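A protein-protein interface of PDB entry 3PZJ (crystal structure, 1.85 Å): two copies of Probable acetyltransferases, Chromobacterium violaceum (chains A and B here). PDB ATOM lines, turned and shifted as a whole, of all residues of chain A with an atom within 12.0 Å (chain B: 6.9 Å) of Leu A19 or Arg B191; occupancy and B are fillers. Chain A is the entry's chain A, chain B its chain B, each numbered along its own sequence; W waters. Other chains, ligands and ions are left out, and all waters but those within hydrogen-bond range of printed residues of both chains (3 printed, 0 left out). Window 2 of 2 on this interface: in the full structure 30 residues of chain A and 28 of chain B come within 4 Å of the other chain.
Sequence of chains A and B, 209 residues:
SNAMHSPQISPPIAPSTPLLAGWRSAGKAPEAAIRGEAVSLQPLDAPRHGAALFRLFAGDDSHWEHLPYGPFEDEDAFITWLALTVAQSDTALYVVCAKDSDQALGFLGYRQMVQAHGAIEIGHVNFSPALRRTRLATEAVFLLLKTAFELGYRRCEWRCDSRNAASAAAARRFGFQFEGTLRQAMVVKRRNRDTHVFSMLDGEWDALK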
ATOM      1  N   ALA A  14     -15.254   8.280 -27.507  1.00  0.00           N
ATOM      2  CA  ALA A  14     -13.818   8.219 -27.713  1.00  0.00           C
ATOM      3  C   ALA A  14     -13.529   7.273 -28.894  1.00  0.00           C
ATOM      4  O   ALA A  14     -14.135   6.185 -28.992  1.00  0.00           O
ATOM      5  CB  ALA A  14     -13.122   7.744 -26.459  1.00  0.00           C
ATOM      6  N   PRO A  15     -12.594   7.676 -29.793  1.00  0.00           N
ATOM      7  CA  PRO A  15     -12.178   6.765 -30.864  1.00  0.00           C
ATOM      8  C   PRO A  15     -11.291   5.601 -30.382  1.00  0.00           C
ATOM      9  O   PRO A  15     -10.885   5.554 -29.218  1.00  0.00           O
ATOM     10  CB  PRO A  15     -11.336   7.692 -31.779  1.00  0.00           C
ATOM     11  CG  PRO A  15     -10.649   8.618 -30.803  1.00  0.00           C
ATOM     12  CD  PRO A  15     -11.727   8.883 -29.729  1.00  0.00           C
ATOM     13  N   SER A  16     -10.914   4.718 -31.317  1.00  0.00           N
ATOM     14  CA  SER A  16      -9.905   3.701 -31.053  1.00  0.00           C
ATOM     15  C   SER A  16      -8.556   4.377 -30.769  1.00  0.00           C
ATOM     16  O   SER A  16      -8.274   5.425 -31.339  1.00  0.00           O
ATOM     17  CB  SER A  16      -9.747   2.773 -32.239  1.00  0.00           C
ATOM     18  OG  SER A  16      -9.124   1.581 -31.802  1.00  0.00           O
ATOM     19  N   THR A  17      -7.765   3.813 -29.854  1.00  0.00           N
ATOM     20  CA  THR A  17      -6.409   4.310 -29.611  1.00  0.00           C
ATOM     21  C   THR A  17      -5.371   3.177 -29.611  1.00  0.00           C
ATOM     22  O   THR A  17      -5.701   2.009 -29.447  1.00  0.00           O
ATOM     23  CB  THR A  17      -6.300   5.155 -28.289  1.00  0.00           C
ATOM     24  OG1 THR A  17      -6.962   4.468 -27.234  1.00  0.00           O
ATOM     25  CG2 THR A  17      -6.873   6.598 -28.462  1.00  0.00           C
ATOM     26  N   PRO A  18      -4.103   3.526 -29.833  1.00  0.00           N
ATOM     27  CA  PRO A  18      -3.130   2.464 -29.860  1.00  0.00           C
ATOM     28  C   PRO A  18      -2.992   1.759 -28.521  1.00  0.00           C
ATOM     29  O   PRO A  18      -3.411   2.270 -27.496  1.00  0.00           O
ATOM     30  CB  PRO A  18      -1.827   3.192 -30.222  1.00  0.00           C
ATOM     31  CG  PRO A  18      -2.017   4.572 -29.737  1.00  0.00           C
ATOM     32  CD  PRO A  18      -3.462   4.839 -30.083  1.00  0.00           C
ATOM     33  N   LEU A  19      -2.445   0.574 -28.564  1.00  0.00           N
ATOM     34  CA  LEU A  19      -2.001  -0.106 -27.366  1.00  0.00           C
ATOM     35  C   LEU A  19      -1.019   0.762 -26.574  1.00  0.00           C
ATOM     36  O   LEU A  19      -0.238   1.547 -27.156  1.00  0.00           O
ATOM     37  CB  LEU A  19      -1.305  -1.394 -27.738  1.00  0.00           C
ATOM     38  CG  LEU A  19      -2.137  -2.670 -27.657  1.00  0.00           C
ATOM     39  CD1 LEU A  19      -3.128  -2.666 -28.823  1.00  0.00           C
ATOM     40  CD2 LEU A  19      -1.227  -3.880 -27.637  1.00  0.00           C
ATOM     41  N   LEU A  20      -1.064   0.604 -25.250  1.00  0.00           N
ATOM     42  CA  LEU A  20      -0.097   1.235 -24.362  1.00  0.00           C
ATOM     43  C   LEU A  20       1.151   0.381 -24.327  1.00  0.00           C
ATOM     44  O   LEU A  20       1.026  -0.834 -24.048  1.00  0.00           O
ATOM     45  CB  LEU A  20      -0.642   1.332 -22.938  1.00  0.00           C
ATOM     46  CG  LEU A  20      -1.883   2.176 -22.835  1.00  0.00           C
ATOM     47  CD1 LEU A  20      -2.581   2.070 -21.440  1.00  0.00           C
ATOM     48  CD2 LEU A  20      -1.525   3.617 -23.166  1.00  0.00           C
ATOM     49  N   ALA A  21       2.322   1.014 -24.568  1.00  0.00           N
ATOM     50  CA  ALA A  21       3.605   0.276 -24.684  1.00  0.00           C
ATOM     51  C   ALA A  21       4.189  -0.011 -23.303  1.00  0.00           C
ATOM     52  O   ALA A  21       4.284   0.892 -22.437  1.00  0.00           O
ATOM     53  CB  ALA A  21       4.626   1.061 -25.540  1.00  0.00           C
ATOM     54  N   GLY A  22       4.554  -1.262 -23.087  1.00  0.00           N
ATOM     55  CA  GLY A  22       5.201  -1.649 -21.861  1.00  0.00           C
ATOM     56  C   GLY A  22       4.289  -1.428 -20.663  1.00  0.00           C
ATOM     57  O   GLY A  22       4.784  -1.057 -19.575  1.00  0.00           O
ATOM     58  N   TRP A  23       2.978  -1.636 -20.847  1.00  0.00           N
ATOM     59  CA  TRP A  23       2.055  -1.571 -19.701  1.00  0.00           C
ATOM     60  C   TRP A  23       2.302  -2.753 -18.756  1.00  0.00           C
ATOM     61  O   TRP A  23       2.501  -3.903 -19.191  1.00  0.00           O
ATOM     62  CB  TRP A  23       0.575  -1.554 -20.125  1.00  0.00           C
ATOM     63  CG  TRP A  23      -0.294  -1.717 -18.933  1.00  0.00           C
ATOM     64  CD1 TRP A  23      -1.028  -2.826 -18.607  1.00  0.00           C
ATOM     65  CD2 TRP A  23      -0.374  -0.831 -17.798  1.00  0.00           C
ATOM     66  NE1 TRP A  23      -1.614  -2.653 -17.375  1.00  0.00           N
ATOM     67  CE2 TRP A  23      -1.262  -1.426 -16.868  1.00  0.00           C
ATOM     68  CE3 TRP A  23       0.203   0.414 -17.488  1.00  0.00           C
ATOM     69  CZ2 TRP A  23      -1.564  -0.851 -15.646  1.00  0.00           C
ATOM     70  CZ3 TRP A  23      -0.139   1.015 -16.273  1.00  0.00           C
ATOM     71  CH2 TRP A  23      -0.992   0.363 -15.367  1.00  0.00           C
ATOM     72  N   ARG A  24       2.370  -2.466 -17.470  1.00  0.00           N
ATOM     73  CA  ARG A  24       2.313  -3.506 -16.439  1.00  0.00           C
ATOM     74  C   ARG A  24       1.655  -2.954 -15.177  1.00  0.00           C
ATOM     75  O   ARG A  24       1.519  -1.704 -15.052  1.00  0.00           O
ATOM     76  CB  ARG A  24       3.679  -3.994 -16.074  1.00  0.00           C
ATOM     77  CG  ARG A  24       4.566  -2.982 -15.400  1.00  0.00           C
ATOM     78  CD  ARG A  24       5.876  -3.695 -15.156  1.00  0.00           C
ATOM     79  NE  ARG A  24       6.917  -2.796 -14.714  1.00  0.00           N
ATOM     80  CZ  ARG A  24       7.660  -2.969 -13.626  1.00  0.00           C
ATOM     81  NH1 ARG A  24       7.521  -4.029 -12.830  1.00  0.00           N
ATOM     82  NH2 ARG A  24       8.577  -2.059 -13.340  1.00  0.00           N
ATOM     83  N   SER A  25       1.290  -3.841 -14.243  1.00  0.00           N
ATOM     84  CA  SER A  25       0.693  -3.356 -13.009  1.00  0.00           C
ATOM     85  C   SER A  25       1.624  -2.378 -12.308  1.00  0.00           C
ATOM     86  O   SER A  25       2.870  -2.512 -12.334  1.00  0.00           O
ATOM     87  CB  SER A  25       0.357  -4.458 -12.049  1.00  0.00           C
ATOM     88  OG  SER A  25      -0.609  -5.333 -12.637  1.00  0.00           O
ATOM     89  N   GLN A 115      -3.682  -1.505  -8.366  1.00  0.00           N
ATOM     90  CA  GLN A 115      -2.421  -1.714  -9.086  1.00  0.00           C
ATOM     91  C   GLN A 115      -2.621  -2.126 -10.501  1.00  0.00           C
ATOM     92  O   GLN A 115      -1.956  -1.596 -11.410  1.00  0.00           O
ATOM     93  CB  GLN A 115      -1.515  -2.782  -8.401  1.00  0.00           C
ATOM     94  CG  GLN A 115      -1.117  -2.374  -7.009  1.00  0.00           C
ATOM     95  CD  GLN A 115      -0.305  -3.382  -6.331  1.00  0.00           C
ATOM     96  OE1 GLN A 115      -0.812  -4.105  -5.479  1.00  0.00           O
ATOM     97  NE2 GLN A 115       0.938  -3.518  -6.739  1.00  0.00           N
ATOM     98  N   ALA A 116      -3.593  -3.003 -10.730  1.00  0.00           N
ATOM     99  CA  ALA A 116      -3.842  -3.569 -12.093  1.00  0.00           C
ATOM    100  C   ALA A 116      -4.251  -2.505 -13.118  1.00  0.00           C
ATOM    101  O   ALA A 116      -4.030  -2.683 -14.291  1.00  0.00           O
ATOM    102  CB  ALA A 116      -4.893  -4.756 -12.038  1.00  0.00           C
ATOM    103  N   HIS A 117      -4.821  -1.380 -12.658  1.00  0.00           N
ATOM    104  CA  HIS A 117      -5.251  -0.299 -13.573  1.00  0.00           C
ATOM    105  C   HIS A 117      -4.452   0.952 -13.484  1.00  0.00           C
ATOM    106  O   HIS A 117      -4.722   1.910 -14.209  1.00  0.00           O
ATOM    107  CB  HIS A 117      -6.712  -0.019 -13.283  1.00  0.00           C
ATOM    108  CG  HIS A 117      -7.554  -1.105 -13.809  1.00  0.00           C
ATOM    109  ND1 HIS A 117      -7.497  -1.437 -15.142  1.00  0.00           N
ATOM    110  CD2 HIS A 117      -8.315  -2.055 -13.205  1.00  0.00           C
ATOM    111  CE1 HIS A 117      -8.246  -2.511 -15.351  1.00  0.00           C
ATOM    112  NE2 HIS A 117      -8.770  -2.889 -14.204  1.00  0.00           N
ATOM    113  N   GLY A 118      -3.476   0.945 -12.586  1.00  0.00           N
ATOM    114  CA  GLY A 118      -2.613   2.086 -12.346  1.00  0.00           C
ATOM    115  C   GLY A 118      -3.406   3.284 -11.857  1.00  0.00           C
ATOM    116  O   GLY A 118      -3.117   4.459 -12.230  1.00  0.00           O
ATOM    117  N   ALA A 119      -4.391   3.017 -11.020  1.00  0.00           N
ATOM    118  CA  ALA A 119      -5.215   4.085 -10.491  1.00  0.00           C
ATOM    119  C   ALA A 119      -5.042   4.097  -8.980  1.00  0.00           C
ATOM    120  O   ALA A 119      -5.090   3.032  -8.313  1.00  0.00           O
ATOM    121  CB  ALA A 119      -6.741   3.892 -10.865  1.00  0.00           C
ATOM    122  N   ARG A 154      -1.019   5.688 -13.443  1.00  0.00           N
ATOM    123  CA  ARG A 154      -1.479   6.520 -14.588  1.00  0.00           C
ATOM    124  C   ARG A 154      -2.431   7.644 -14.190  1.00  0.00           C
ATOM    125  O   ARG A 154      -2.551   8.623 -14.893  1.00  0.00           O
ATOM    126  CB  ARG A 154      -2.224   5.628 -15.604  1.00  0.00           C
ATOM    127  CG  ARG A 154      -1.366   4.617 -16.250  1.00  0.00           C
ATOM    128  CD  ARG A 154      -2.105   3.805 -17.279  1.00  0.00           C
ATOM    129  NE  ARG A 154      -2.350   4.588 -18.421  1.00  0.00           N
ATOM    130  CZ  ARG A 154      -3.521   4.811 -18.990  1.00  0.00           C
ATOM    131  NH1 ARG A 154      -4.635   4.381 -18.472  1.00  0.00           N
ATOM    132  NH2 ARG A 154      -3.554   5.585 -20.082  1.00  0.00           N
ATOM    133  N   ARG A 155      -3.090   7.505 -13.056  1.00  0.00           N
ATOM    134  CA  ARG A 155      -4.134   8.404 -12.629  1.00  0.00           C
ATOM    135  C   ARG A 155      -4.058   8.512 -11.079  1.00  0.00           C
ATOM    136  O   ARG A 155      -4.071   7.467 -10.402  1.00  0.00           O
ATOM    137  CB  ARG A 155      -5.485   7.768 -13.012  1.00  0.00           C
ATOM    138  CG  ARG A 155      -6.722   8.525 -12.495  1.00  0.00           C
ATOM    139  CD  ARG A 155      -8.003   7.707 -12.630  1.00  0.00           C
ATOM    140  NE  ARG A 155      -9.138   8.343 -11.990  1.00  0.00           N
ATOM    141  CZ  ARG A 155      -9.699   9.525 -12.373  1.00  0.00           C
ATOM    142  NH1 ARG A 155      -9.349  10.170 -13.468  1.00  0.00           N
ATOM    143  NH2 ARG A 155     -10.632  10.056 -11.634  1.00  0.00           N
ATOM    144  N   ASP A 202      -0.705  10.840 -15.608  1.00  0.00           N
ATOM    145  CA  ASP A 202       0.720  10.698 -15.747  1.00  0.00           C
ATOM    146  C   ASP A 202       1.291  11.727 -16.733  1.00  0.00           C
ATOM    147  O   ASP A 202       2.362  12.257 -16.511  1.00  0.00           O
ATOM    148  CB  ASP A 202       1.163   9.256 -16.073  1.00  0.00           C
ATOM    149  CG  ASP A 202       0.492   8.607 -17.278  1.00  0.00           C
ATOM    150  OD1 ASP A 202      -0.384   9.192 -17.899  1.00  0.00           O
ATOM    151  OD2 ASP A 202       0.867   7.429 -17.590  1.00  0.00           O
ATOM    152  N   ASP B 161     -17.199   2.512 -20.600  1.00  0.00           N
ATOM    153  CA  ASP B 161     -15.980   2.945 -21.292  1.00  0.00           C
ATOM    154  C   ASP B 161     -16.434   4.071 -22.186  1.00  0.00           C
ATOM    155  O   ASP B 161     -17.421   3.877 -22.852  1.00  0.00           O
ATOM    156  CB  ASP B 161     -15.469   1.776 -22.131  1.00  0.00           C
ATOM    157  CG  ASP B 161     -14.158   2.034 -22.739  1.00  0.00           C
ATOM    158  OD1 ASP B 161     -14.038   3.040 -23.418  1.00  0.00           O
ATOM    159  OD2 ASP B 161     -13.261   1.174 -22.581  1.00  0.00           O
ATOM    160  N   ARG B 163     -15.560   4.727 -25.047  1.00  0.00           N
ATOM    161  CA  ARG B 163     -15.691   4.201 -26.458  1.00  0.00           C
ATOM    162  C   ARG B 163     -17.015   3.531 -26.726  1.00  0.00           C
ATOM    163  O   ARG B 163     -17.286   3.158 -27.861  1.00  0.00           O
ATOM    164  CB  ARG B 163     -14.567   3.187 -26.781  1.00  0.00           C
ATOM    165  CG  ARG B 163     -13.107   3.775 -26.641  1.00  0.00           C
ATOM    166  CD  ARG B 163     -12.014   2.719 -26.787  1.00  0.00           C
ATOM    167  NE  ARG B 163     -11.914   1.963 -25.523  1.00  0.00           N
ATOM    168  CZ  ARG B 163     -11.250   0.818 -25.350  1.00  0.00           C
ATOM    169  NH1 ARG B 163     -11.263   0.238 -24.154  1.00  0.00           N
ATOM    170  NH2 ARG B 163     -10.565   0.249 -26.361  1.00  0.00           N
ATOM    171  N   MET B 186      -8.816   3.098 -16.257  1.00  0.00           N
ATOM    172  CA  MET B 186      -8.457   1.678 -16.385  1.00  0.00           C
ATOM    173  C   MET B 186      -7.597   1.430 -17.647  1.00  0.00           C
ATOM    174  O   MET B 186      -7.515   2.275 -18.521  1.00  0.00           O
ATOM    175  CB  MET B 186      -9.762   0.857 -16.475  1.00  0.00           C
ATOM    176  CG  MET B 186     -10.564   0.924 -15.168  1.00  0.00           C
ATOM    177  SD  MET B 186     -12.277  -0.030 -15.528  1.00  0.00           S
ATOM    178  CE  MET B 186     -11.540  -1.645 -15.681  1.00  0.00           C
ATOM    179  N   VAL B 187      -6.888   0.304 -17.627  1.00  0.00           N
ATOM    180  CA  VAL B 187      -6.181  -0.275 -18.833  1.00  0.00           C
ATOM    181  C   VAL B 187      -6.929  -1.565 -19.078  1.00  0.00           C
ATOM    182  O   VAL B 187      -6.939  -2.446 -18.201  1.00  0.00           O
ATOM    183  CB  VAL B 187      -4.734  -0.494 -18.564  1.00  0.00           C
ATOM    184  CG1 VAL B 187      -4.020  -1.098 -19.745  1.00  0.00           C
ATOM    185  CG2 VAL B 187      -4.111   0.900 -18.278  1.00  0.00           C
ATOM    186  N   VAL B 188      -7.617  -1.609 -20.205  1.00  0.00           N
ATOM    187  CA  VAL B 188      -8.430  -2.742 -20.626  1.00  0.00           C
ATOM    188  C   VAL B 188      -7.805  -3.313 -21.886  1.00  0.00           C
ATOM    189  O   VAL B 188      -7.781  -2.619 -22.905  1.00  0.00           O
ATOM    190  CB  VAL B 188      -9.914  -2.299 -20.860  1.00  0.00           C
ATOM    191  CG1 VAL B 188     -10.827  -3.497 -21.235  1.00  0.00           C
ATOM    192  CG2 VAL B 188     -10.570  -1.601 -19.596  1.00  0.00           C
ATOM    193  N   LYS B 189      -7.279  -4.553 -21.802  1.00  0.00           N
ATOM    194  CA  LYS B 189      -6.638  -5.221 -22.896  1.00  0.00           C
ATOM    195  C   LYS B 189      -5.550  -4.298 -23.488  1.00  0.00           C
ATOM    196  O   LYS B 189      -5.567  -4.050 -24.684  1.00  0.00           O
ATOM    197  CB  LYS B 189      -7.693  -5.573 -23.940  1.00  0.00           C
ATOM    198  N   ARG B 190      -4.675  -3.783 -22.611  1.00  0.00           N
ATOM    199  CA  ARG B 190      -3.509  -2.962 -22.969  1.00  0.00           C
ATOM    200  C   ARG B 190      -3.877  -1.633 -23.685  1.00  0.00           C
ATOM    201  O   ARG B 190      -2.940  -0.953 -24.207  1.00  0.00           O
ATOM    202  CB  ARG B 190      -2.399  -3.745 -23.721  1.00  0.00           C
ATOM    203  CG  ARG B 190      -1.691  -4.868 -22.906  1.00  0.00           C
ATOM    204  CD  ARG B 190      -0.458  -5.561 -23.668  1.00  0.00           C
ATOM    205  NE  ARG B 190       0.147  -6.553 -22.762  1.00  0.00           N
ATOM    206  CZ  ARG B 190       1.027  -6.268 -21.789  1.00  0.00           C
ATOM    207  NH1 ARG B 190       1.460  -7.258 -20.989  1.00  0.00           N
ATOM    208  NH2 ARG B 190       1.565  -5.022 -21.668  1.00  0.00           N
ATOM    209  N   ARG B 191      -5.183  -1.245 -23.655  1.00  0.00           N
ATOM    210  CA  ARG B 191      -5.649   0.082 -24.178  1.00  0.00           C
ATOM    211  C   ARG B 191      -6.189   1.010 -23.068  1.00  0.00           C
ATOM    212  O   ARG B 191      -6.693   0.539 -22.050  1.00  0.00           O
ATOM    213  CB  ARG B 191      -6.730  -0.048 -25.191  1.00  0.00           C
ATOM    214  CG  ARG B 191      -6.222  -0.645 -26.508  1.00  0.00           C
ATOM    215  CD  ARG B 191      -7.274  -0.429 -27.589  1.00  0.00           C
ATOM    216  NE  ARG B 191      -6.657  -0.737 -28.867  1.00  0.00           N
ATOM    217  CZ  ARG B 191      -6.481  -1.967 -29.315  1.00  0.00           C
ATOM    218  NH1 ARG B 191      -6.934  -3.011 -28.629  1.00  0.00           N
ATOM    219  NH2 ARG B 191      -5.872  -2.145 -30.478  1.00  0.00           N
ATOM    220  N   ASN B 192      -6.103   2.319 -23.293  1.00  0.00           N
ATOM    221  CA  ASN B 192      -6.685   3.258 -22.359  1.00  0.00           C
ATOM    222  C   ASN B 192      -8.215   3.143 -22.230  1.00  0.00           C
ATOM    223  O   ASN B 192      -8.915   3.019 -23.233  1.00  0.00           O
ATOM    224  CB  ASN B 192      -6.402   4.691 -22.767  1.00  0.00           C
ATOM    225  CG  ASN B 192      -6.925   5.698 -21.703  1.00  0.00           C
ATOM    226  OD1 ASN B 192      -6.487   5.701 -20.555  1.00  0.00           O
ATOM    227  ND2 ASN B 192      -7.902   6.469 -22.069  1.00  0.00           N
ATOM    228  N   ARG B 193      -8.720   3.304 -21.022  1.00  0.00           N
ATOM    229  CA  ARG B 193     -10.131   3.497 -20.817  1.00  0.00           C
ATOM    230  C   ARG B 193     -10.442   4.746 -19.980  1.00  0.00           C
ATOM    231  O   ARG B 193      -9.997   4.863 -18.893  1.00  0.00           O
ATOM    232  CB  ARG B 193     -10.785   2.291 -20.121  1.00  0.00           C
ATOM    233  CG  ARG B 193     -12.154   2.644 -19.560  1.00  0.00           C
ATOM    234  CD  ARG B 193     -12.986   1.471 -19.165  1.00  0.00           C
ATOM    235  NE  ARG B 193     -14.081   1.843 -18.316  1.00  0.00           N
ATOM    236  CZ  ARG B 193     -15.126   1.097 -18.026  1.00  0.00           C
ATOM    237  NH1 ARG B 193     -16.044   1.567 -17.224  1.00  0.00           N
ATOM    238  NH2 ARG B 193     -15.255  -0.108 -18.519  1.00  0.00           N
HETATM  239  O   HOH W   1      -5.377   3.495 -15.947  1.00  0.00           O
HETATM  240  O   HOH W   2     -10.252   0.934 -29.443  1.00  0.00           O
HETATM  241  O   HOH W   3      -4.750   3.340 -25.534  1.00  0.00           O
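O of Thr A17 sits at hydrogen-bond distance from NE of Arg B191 (3.0 Å). N of Leu A20 lies within hydrogen-bond range of O of Arg B190 (2.7 Å). The backbone carbonyl oxygen of Trp A23 lies within hydrogen-bond range of the guanidinium group of Arg B190 (2.9 Å). ND1 of His A117 is in hydrogen-bond range of N of Val B187, at 3.1 Å. The guanidinium group (NH2) of Arg A154 sits at hydrogen-bond distance from the side-chain amide oxygen (OD1) of Asn B192.
The backbone carbonyl oxygen of Gly A118 is in hydrogen-bond range of the backbone NH of Arg A154 (2.7 Å). The backbone carbonyl oxygen (O) of Arg A154 lies within hydrogen-bond range of the backbone NH (N) of Asp A202 (3.0 Å). The guanidinium group (NH1) of Arg B163 is in salt-bridge range of the side-chain carboxylate (OD2) of Asp B161. The backbone carbonyl oxygen (O) of Met B186 is in hydrogen-bond range of the backbone NH (N) of Arg B193 (3.0 Å).
Among the printed residues, pairs that only touch across the chains: Leu A19 with Arg B191 (3.2 Å), His A117 with Met B186 (3.4 Å), Leu A19 with Arg B190 (3.4 Å), Ala A14 with Arg B163 (3.5 Å), Arg A154 with Val B187 (3.5 Å), Arg A154 with Met B186 (3.6 Å), Trp A23 with Val B187 (3.6 Å), Leu A20 with Val B187 (3.7 Å), Pro A15 with Arg B163 (3.8 Å) and Leu A20 with Asn B192 (3.99 Å).
Printed residues of chain B within 4 Å of Pro A15: Arg B163 (3.8 Å). Of chain B, only Arg B190 and Arg B191 come within 4 Å of Leu A19. Printed residues of chain B within 4 Å of Leu A20: Val B187 (3.7 Å), Arg B190 (2.7 Å) and Asn B192 (3.99 Å). Gly A22 touches none of the printed residues of chain B. Of the printed residues of chain B, His A117 touches Met B186 and Val B187. Gly A118 touches none of the printed residues of chain B. Printed residues of chain A within 4 Å of Arg B163: Ala A14 (3.5 Å) and Pro A15 (3.8 Å). No residue of chain A comes within 4 Å of Val B188. No residue of chain A comes within 4 Å of Lys B189. Of the printed residues of chain A, Arg B190 touches Leu A19, Leu A20 and Trp A23. Arg B191 touches just these residues of chain A: Thr A17 (3.0 Å) and Leu A19 (3.2 Å). The nearest residue of chain B that does not touch Leu A19 is Lys B189 (4.7 Å). The nearest printed residue of chain A that does not touch Asn B192 is Thr A17 (4.5 Å).
Of the 10 printed residues of chain B, 6 touch a printed residue of chain A. Hydrophobic or aromatic side chains of chain B that line the printed part of chain A: Met B186 and Val B187. Of the 20 printed residues of chain A, 8 touch a printed residue of chain B. Hydrophobic or aromatic side chains of chain A within 4 Å of the printed part of chain B: Ala A14, Leu A19, Leu A20, Trp A23 and His A117. Among the printed residues, 15 pairs touch across the chains.
No position is printed for both chains. Of the 15 pairs that touch across the chains among the printed residues, none has its exchanged pair printed and touching as well.
Water W1 lies within hydrogen-bond range of O of His A117 (2.4 Å), NH1 of Arg A154 (2.8 Å) and N of Met B186 (3.5 Å). Water W3 lies within hydrogen-bond range of O of Pro A18 (2.6 Å), N of Asn B192 (2.8 Å) and OG1 of Thr A17 (3.0 Å). Water W2 bridges the side-chain hydroxyl (OG) of Ser A16 (2.7 Å) and the guanidinium group (NH2) of Arg B163 (3.2 Å).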
